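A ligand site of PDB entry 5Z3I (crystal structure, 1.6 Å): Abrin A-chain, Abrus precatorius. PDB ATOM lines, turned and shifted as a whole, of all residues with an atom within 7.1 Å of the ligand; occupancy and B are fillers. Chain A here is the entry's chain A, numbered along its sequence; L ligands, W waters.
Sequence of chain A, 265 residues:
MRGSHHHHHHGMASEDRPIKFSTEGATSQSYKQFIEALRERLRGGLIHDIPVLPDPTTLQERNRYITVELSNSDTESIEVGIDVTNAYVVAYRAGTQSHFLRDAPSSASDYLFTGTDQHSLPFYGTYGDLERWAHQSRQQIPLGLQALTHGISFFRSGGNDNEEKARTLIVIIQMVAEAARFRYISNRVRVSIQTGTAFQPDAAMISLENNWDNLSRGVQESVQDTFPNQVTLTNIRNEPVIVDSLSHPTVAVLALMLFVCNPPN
Water W2 lies within hydrogen-bond range of a nitrogen (N1) of the ligand (2.8 Å), the side-chain carboxylate (OE2) of Glu 178 (2.8 Å) and the backbone carbonyl oxygen (O) of Glu 209 (3.4 Å).
The backbone carbonyl oxygen (O) of Gly 125 is in hydrogen-bond range of a nitrogen (N3) of the ligand. The backbone NH (N) of Val 89 is in hydrogen-bond range of a nitrogen (N4) of the ligand, 2.9 Å away. N3 of the ligand is in hydrogen-bond range of O of Val 89 (3.1 Å). The guanidinium group (NH1) of Arg 181 lies within hydrogen-bond range of a nitrogen (N5) of the ligand (2.9 Å).
Merely in contact with the ligand: Ala 87 (3.6 Å), Tyr 88 (3.3 Å), Tyr 127 (3.7 Å), Ile 173 (3.3 Å), Ala 177 (3.7 Å) and Glu 178 (3.9 Å). Hydrophobic or aromatic side chains within 4 Å of the ligand: Tyr 88, Val 89, Tyr 127, Ile 173 and Ala 177. Of the 21 residues printed, 9 come within 4 Å of the ligand.
N of Gly 125 lies within hydrogen-bond range of OD1 of Asp 103 (2.8 Å). NH1 of Arg 181 is in salt-bridge range of OE1 of Glu 178, at 3.0 Å. NH2 of Arg 181 is in hydrogen-bond range of O of Asn 86 (2.7 Å). N of Tyr 88 is in hydrogen-bond range of OD1 of Asn 86, 3.0 Å away. The backbone carbonyl oxygen of Ile 173 sits at hydrogen-bond distance from the backbone NH of Glu 178 (3.0 Å). The side-chain hydroxyl of Tyr 127 is in hydrogen-bond range of the side-chain carboxylate of Glu 178 (2.6 Å).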
ATOM      1  N   ASN A  86      23.564  25.732   0.549  1.00  0.00           N
ATOM      2  CA  ASN A  86      22.556  26.077   1.529  1.00  0.00           C
ATOM      3  C   ASN A  86      22.959  27.264   2.397  1.00  0.00           C
ATOM      4  O   ASN A  86      22.243  27.558   3.362  1.00  0.00           O
ATOM      5  CB  ASN A  86      22.231  24.852   2.402  1.00  0.00           C
ATOM      6  CG  ASN A  86      23.469  24.248   3.046  1.00  0.00           C
ATOM      7  OD1 ASN A  86      24.540  24.843   3.049  1.00  0.00           O
ATOM      8  ND2 ASN A  86      23.315  23.045   3.600  1.00  0.00           N
ATOM      9  N   ALA A  87      24.068  27.939   2.077  1.00  0.00           N
ATOM     10  CA  ALA A  87      24.576  29.088   2.835  1.00  0.00           C
ATOM     11  C   ALA A  87      24.911  28.702   4.273  1.00  0.00           C
ATOM     12  O   ALA A  87      24.940  29.560   5.168  1.00  0.00           O
ATOM     13  CB  ALA A  87      23.601  30.264   2.809  1.00  0.00           C
ATOM     14  N   TYR A  88      25.183  27.427   4.523  1.00  0.00           N
ATOM     15  CA  TYR A  88      25.527  26.992   5.871  1.00  0.00           C
ATOM     16  C   TYR A  88      26.980  27.313   6.186  1.00  0.00           C
ATOM     17  O   TYR A  88      27.878  27.141   5.354  1.00  0.00           O
ATOM     18  CB  TYR A  88      25.284  25.491   6.051  1.00  0.00           C
ATOM     19  CG  TYR A  88      23.936  25.180   6.649  1.00  0.00           C
ATOM     20  CD1 TYR A  88      22.771  25.617   6.045  1.00  0.00           C
ATOM     21  CD2 TYR A  88      23.831  24.464   7.845  1.00  0.00           C
ATOM     22  CE1 TYR A  88      21.530  25.339   6.596  1.00  0.00           C
ATOM     23  CE2 TYR A  88      22.600  24.196   8.401  1.00  0.00           C
ATOM     24  CZ  TYR A  88      21.449  24.636   7.780  1.00  0.00           C
ATOM     25  OH  TYR A  88      20.222  24.356   8.331  1.00  0.00           O
ATOM     26  N   VAL A  89      27.195  27.829   7.393  1.00  0.00           N
ATOM     27  CA  VAL A  89      28.527  27.826   7.987  1.00  0.00           C
ATOM     28  C   VAL A  89      28.869  26.395   8.364  1.00  0.00           C
ATOM     29  O   VAL A  89      28.156  25.760   9.150  1.00  0.00           O
ATOM     30  CB  VAL A  89      28.586  28.754   9.211  1.00  0.00           C
ATOM     31  CG1 VAL A  89      29.947  28.642   9.899  1.00  0.00           C
ATOM     32  CG2 VAL A  89      28.293  30.182   8.805  1.00  0.00           C
ATOM     33  N   VAL A  90      29.958  25.877   7.800  1.00  0.00           N
ATOM     34  CA  VAL A  90      30.360  24.502   8.054  1.00  0.00           C
ATOM     35  C   VAL A  90      31.684  24.412   8.793  1.00  0.00           C
ATOM     36  O   VAL A  90      32.028  23.312   9.269  1.00  0.00           O
ATOM     37  CB  VAL A  90      30.446  23.685   6.743  1.00  0.00           C
ATOM     38  CG1 VAL A  90      29.076  23.618   6.091  1.00  0.00           C
ATOM     39  CG2 VAL A  90      31.491  24.271   5.796  1.00  0.00           C
ATOM     40  N   LEU A 101      32.009  21.797  11.890  1.00  0.00           N
ATOM     41  CA  LEU A 101      30.793  21.324  12.528  1.00  0.00           C
ATOM     42  C   LEU A 101      30.662  19.813  12.359  1.00  0.00           C
ATOM     43  O   LEU A 101      31.099  19.238  11.366  1.00  0.00           O
ATOM     44  CB  LEU A 101      29.559  22.041  11.946  1.00  0.00           C
ATOM     45  CG  LEU A 101      29.232  23.435  12.499  1.00  0.00           C
ATOM     46  CD1 LEU A 101      29.059  23.398  14.021  1.00  0.00           C
ATOM     47  CD2 LEU A 101      30.276  24.450  12.096  1.00  0.00           C
ATOM     48  N   ASP A 103      28.257  17.995  11.617  1.00  0.00           N
ATOM     49  CA  ASP A 103      27.473  17.620  10.437  1.00  0.00           C
ATOM     50  C   ASP A 103      27.938  18.339   9.172  1.00  0.00           C
ATOM     51  O   ASP A 103      27.195  18.396   8.188  1.00  0.00           O
ATOM     52  CB  ASP A 103      25.984  17.869  10.681  1.00  0.00           C
ATOM     53  CG  ASP A 103      25.673  19.274  11.203  1.00  0.00           C
ATOM     54  OD1 ASP A 103      26.613  20.070  11.447  1.00  0.00           O
ATOM     55  OD2 ASP A 103      24.472  19.591  11.376  1.00  0.00           O
ATOM     56  N   TYR A 124      26.646  19.652  16.410  1.00  0.00           N
ATOM     57  CA  TYR A 124      26.129  19.893  15.073  1.00  0.00           C
ATOM     58  C   TYR A 124      25.907  21.392  14.848  1.00  0.00           C
ATOM     59  O   TYR A 124      25.804  22.175  15.796  1.00  0.00           O
ATOM     60  CB  TYR A 124      24.803  19.144  14.873  1.00  0.00           C
ATOM     61  CG  TYR A 124      24.920  17.639  15.000  1.00  0.00           C
ATOM     62  CD1 TYR A 124      25.586  16.886  14.054  1.00  0.00           C
ATOM     63  CD2 TYR A 124      24.335  16.961  16.060  1.00  0.00           C
ATOM     64  CE1 TYR A 124      25.690  15.523  14.159  1.00  0.00           C
ATOM     65  CE2 TYR A 124      24.424  15.593  16.182  1.00  0.00           C
ATOM     66  CZ  TYR A 124      25.105  14.874  15.225  1.00  0.00           C
ATOM     67  OH  TYR A 124      25.207  13.505  15.322  1.00  0.00           O
ATOM     68  N   GLY A 125      25.823  21.782  13.580  1.00  0.00           N
ATOM     69  CA  GLY A 125      25.600  23.161  13.214  1.00  0.00           C
ATOM     70  C   GLY A 125      24.149  23.610  13.220  1.00  0.00           C
ATOM     71  O   GLY A 125      23.868  24.728  12.794  1.00  0.00           O
ATOM     72  N   THR A 126      23.237  22.763  13.680  1.00  0.00           N
ATOM     73  CA  THR A 126      21.835  23.121  13.813  1.00  0.00           C
ATOM     74  C   THR A 126      21.636  24.068  14.983  1.00  0.00           C
ATOM     75  O   THR A 126      22.405  24.066  15.954  1.00  0.00           O
ATOM     76  CB  THR A 126      20.989  21.874  14.030  1.00  0.00           C
ATOM     77  OG1 THR A 126      21.372  21.233  15.247  1.00  0.00           O
ATOM     78  CG2 THR A 126      21.152  20.892  12.874  1.00  0.00           C
ATOM     79  N   TYR A 127      20.583  24.892  14.906  1.00  0.00           N
ATOM     80  CA  TYR A 127      20.254  25.747  16.034  1.00  0.00           C
ATOM     81  C   TYR A 127      19.943  24.907  17.275  1.00  0.00           C
ATOM     82  O   TYR A 127      20.331  25.268  18.384  1.00  0.00           O
ATOM     83  CB  TYR A 127      19.087  26.673  15.704  1.00  0.00           C
ATOM     84  CG  TYR A 127      19.454  27.833  14.793  1.00  0.00           C
ATOM     85  CD1 TYR A 127      20.617  28.562  15.018  1.00  0.00           C
ATOM     86  CD2 TYR A 127      18.649  28.182  13.729  1.00  0.00           C
ATOM     87  CE1 TYR A 127      20.969  29.606  14.200  1.00  0.00           C
ATOM     88  CE2 TYR A 127      18.998  29.245  12.901  1.00  0.00           C
ATOM     89  CZ  TYR A 127      20.149  29.951  13.152  1.00  0.00           C
ATOM     90  OH  TYR A 127      20.509  30.999  12.331  1.00  0.00           O
ATOM     91  N   GLY A 128      19.258  23.779  17.082  1.00  0.00           N
ATOM     92  CA  GLY A 128      18.934  22.927  18.204  1.00  0.00           C
ATOM     93  C   GLY A 128      20.161  22.522  19.002  1.00  0.00           C
ATOM     94  O   GLY A 128      20.179  22.629  20.234  1.00  0.00           O
ATOM     95  N   LEU A 130      23.347  23.825  18.688  1.00  0.00           N
ATOM     96  CA  LEU A 130      24.099  24.997  19.125  1.00  0.00           C
ATOM     97  C   LEU A 130      23.464  25.595  20.379  1.00  0.00           C
ATOM     98  O   LEU A 130      24.166  25.916  21.347  1.00  0.00           O
ATOM     99  CB  LEU A 130      24.163  26.020  17.990  1.00  0.00           C
ATOM    100  CG  LEU A 130      25.052  25.650  16.808  1.00  0.00           C
ATOM    101  CD1 LEU A 130      24.848  26.610  15.633  1.00  0.00           C
ATOM    102  CD2 LEU A 130      26.524  25.616  17.223  1.00  0.00           C
ATOM    103  N   LEU A 169      29.134  30.809  17.311  1.00  0.00           N
ATOM    104  CA  LEU A 169      28.632  30.416  16.005  1.00  0.00           C
ATOM    105  C   LEU A 169      27.184  30.867  15.810  1.00  0.00           C
ATOM    106  O   LEU A 169      26.808  31.233  14.682  1.00  0.00           O
ATOM    107  CB  LEU A 169      28.755  28.910  15.805  1.00  0.00           C
ATOM    108  CG  LEU A 169      30.180  28.447  15.438  1.00  0.00           C
ATOM    109  CD1 LEU A 169      30.373  26.946  15.680  1.00  0.00           C
ATOM    110  CD2 LEU A 169      30.500  28.820  13.990  1.00  0.00           C
ATOM    111  N   ILE A 173      26.492  32.894  12.459  1.00  0.00           N
ATOM    112  CA  ILE A 173      25.499  32.332  11.537  1.00  0.00           C
ATOM    113  C   ILE A 173      24.427  33.361  11.214  1.00  0.00           C
ATOM    114  O   ILE A 173      24.023  33.534  10.063  1.00  0.00           O
ATOM    115  CB  ILE A 173      24.900  31.040  12.117  1.00  0.00           C
ATOM    116  CG1 ILE A 173      25.927  29.911  12.072  1.00  0.00           C
ATOM    117  CG2 ILE A 173      23.621  30.640  11.377  1.00  0.00           C
ATOM    118  CD1 ILE A 173      25.527  28.685  12.864  1.00  0.00           C
ATOM    119  N   GLN A 174      23.924  34.060  12.237  1.00  0.00           N
ATOM    120  CA  GLN A 174      22.832  34.988  11.988  1.00  0.00           C
ATOM    121  C   GLN A 174      23.310  36.265  11.319  1.00  0.00           C
ATOM    122  O   GLN A 174      22.627  36.789  10.426  1.00  0.00           O
ATOM    123  CB  GLN A 174      22.113  35.293  13.299  1.00  0.00           C
ATOM    124  CG  GLN A 174      21.366  34.095  13.858  1.00  0.00           C
ATOM    125  CD  GLN A 174      20.744  34.377  15.191  1.00  0.00           C
ATOM    126  OE1 GLN A 174      21.416  34.319  16.233  1.00  0.00           O
ATOM    127  NE2 GLN A 174      19.467  34.694  15.176  1.00  0.00           N
ATOM    128  N   ALA A 177      25.063  34.344   7.536  1.00  0.00           N
ATOM    129  CA  ALA A 177      24.260  33.481   6.668  1.00  0.00           C
ATOM    130  C   ALA A 177      22.785  33.889   6.654  1.00  0.00           C
ATOM    131  O   ALA A 177      22.196  34.033   5.572  1.00  0.00           O
ATOM    132  CB  ALA A 177      24.389  32.028   7.114  1.00  0.00           C
ATOM    133  N   GLU A 178      22.162  34.053   7.822  1.00  0.00           N
ATOM    134  CA  GLU A 178      20.766  34.454   7.835  1.00  0.00           C
ATOM    135  C   GLU A 178      20.596  35.839   7.224  1.00  0.00           C
ATOM    136  O   GLU A 178      19.617  36.111   6.536  1.00  0.00           O
ATOM    137  CB  GLU A 178      20.219  34.439   9.272  1.00  0.00           C
ATOM    138  CG  GLU A 178      20.297  33.084   9.984  1.00  0.00           C
ATOM    139  CD  GLU A 178      19.326  32.045   9.444  1.00  0.00           C
ATOM    140  OE1 GLU A 178      18.753  32.233   8.345  1.00  0.00           O
ATOM    141  OE2 GLU A 178      19.121  31.024  10.155  1.00  0.00           O
ATOM    142  N   ARG A 181      20.456  35.540   3.633  1.00  0.00           N
ATOM    143  CA  ARG A 181      19.214  34.948   3.140  1.00  0.00           C
ATOM    144  C   ARG A 181      18.069  35.942   3.118  1.00  0.00           C
ATOM    145  O   ARG A 181      17.229  35.908   2.214  1.00  0.00           O
ATOM    146  CB  ARG A 181      18.813  33.770   4.009  1.00  0.00           C
ATOM    147  CG  ARG A 181      19.752  32.599   3.991  1.00  0.00           C
ATOM    148  CD  ARG A 181      19.275  31.558   4.990  1.00  0.00           C
ATOM    149  NE  ARG A 181      20.054  30.326   4.903  1.00  0.00           N
ATOM    150  CZ  ARG A 181      20.761  29.802   5.898  1.00  0.00           C
ATOM    151  NH1 ARG A 181      20.796  30.389   7.092  1.00  0.00           N
ATOM    152  NH2 ARG A 181      21.426  28.687   5.702  1.00  0.00           N
ATOM    153  N   GLU A 209      14.117  32.623  10.052  1.00  0.00           N
ATOM    154  CA  GLU A 209      15.176  31.625  10.148  1.00  0.00           C
ATOM    155  C   GLU A 209      14.607  30.210  10.129  1.00  0.00           C
ATOM    156  O   GLU A 209      15.164  29.317   9.492  1.00  0.00           O
ATOM    157  CB  GLU A 209      15.983  31.858  11.419  1.00  0.00           C
ATOM    158  CG  GLU A 209      16.733  33.173  11.446  1.00  0.00           C
ATOM    159  CD  GLU A 209      17.407  33.455  12.780  1.00  0.00           C
ATOM    160  OE1 GLU A 209      17.128  32.728  13.751  1.00  0.00           O
ATOM    161  OE2 GLU A 209      18.195  34.408  12.861  1.00  0.00           O
ATOM    162  N   TRP A 212      12.975  29.111   6.240  1.00  0.00           N
ATOM    163  CA  TRP A 212      13.645  29.406   4.971  1.00  0.00           C
ATOM    164  C   TRP A 212      13.351  28.344   3.932  1.00  0.00           C
ATOM    165  O   TRP A 212      13.028  28.654   2.771  1.00  0.00           O
ATOM    166  CB  TRP A 212      15.130  29.518   5.217  1.00  0.00           C
ATOM    167  CG  TRP A 212      15.945  29.841   4.026  1.00  0.00           C
ATOM    168  CD1 TRP A 212      15.792  30.897   3.173  1.00  0.00           C
ATOM    169  CD2 TRP A 212      17.095  29.124   3.569  1.00  0.00           C
ATOM    170  NE1 TRP A 212      16.772  30.889   2.210  1.00  0.00           N
ATOM    171  CE2 TRP A 212      17.583  29.799   2.433  1.00  0.00           C
ATOM    172  CE3 TRP A 212      17.755  27.981   4.010  1.00  0.00           C
ATOM    173  CZ2 TRP A 212      18.700  29.357   1.726  1.00  0.00           C
ATOM    174  CZ3 TRP A 212      18.850  27.537   3.308  1.00  0.00           C
ATOM    175  CH2 TRP A 212      19.321  28.233   2.185  1.00  0.00           C
HETATM  176  N1  LIG L   1      20.996  27.656  10.230  1.00  0.00           N
HETATM  177  C1  LIG L   1      21.155  26.714  11.202  1.00  0.00           C
HETATM  178  N2  LIG L   1      22.393  26.302  11.336  1.00  0.00           N
HETATM  179  C2  LIG L   1      23.090  27.019  10.377  1.00  0.00           C
HETATM  180  C3  LIG L   1      24.459  27.031   9.998  1.00  0.00           C
HETATM  181  N3  LIG L   1      25.391  26.263  10.563  1.00  0.00           N
HETATM  182  N4  LIG L   1      24.814  27.878   9.014  1.00  0.00           N
HETATM  183  C4  LIG L   1      23.881  28.646   8.449  1.00  0.00           C
HETATM  184  N5  LIG L   1      22.576  28.706   8.707  1.00  0.00           N
HETATM  185  C5  LIG L   1      22.243  27.861   9.686  1.00  0.00           C
HETATM  186  O   HOH W   1      18.772  24.663  12.534  1.00  0.00           O
HETATM  187  O   HOH W   2      18.408  28.351   9.551  1.00  0.00           O
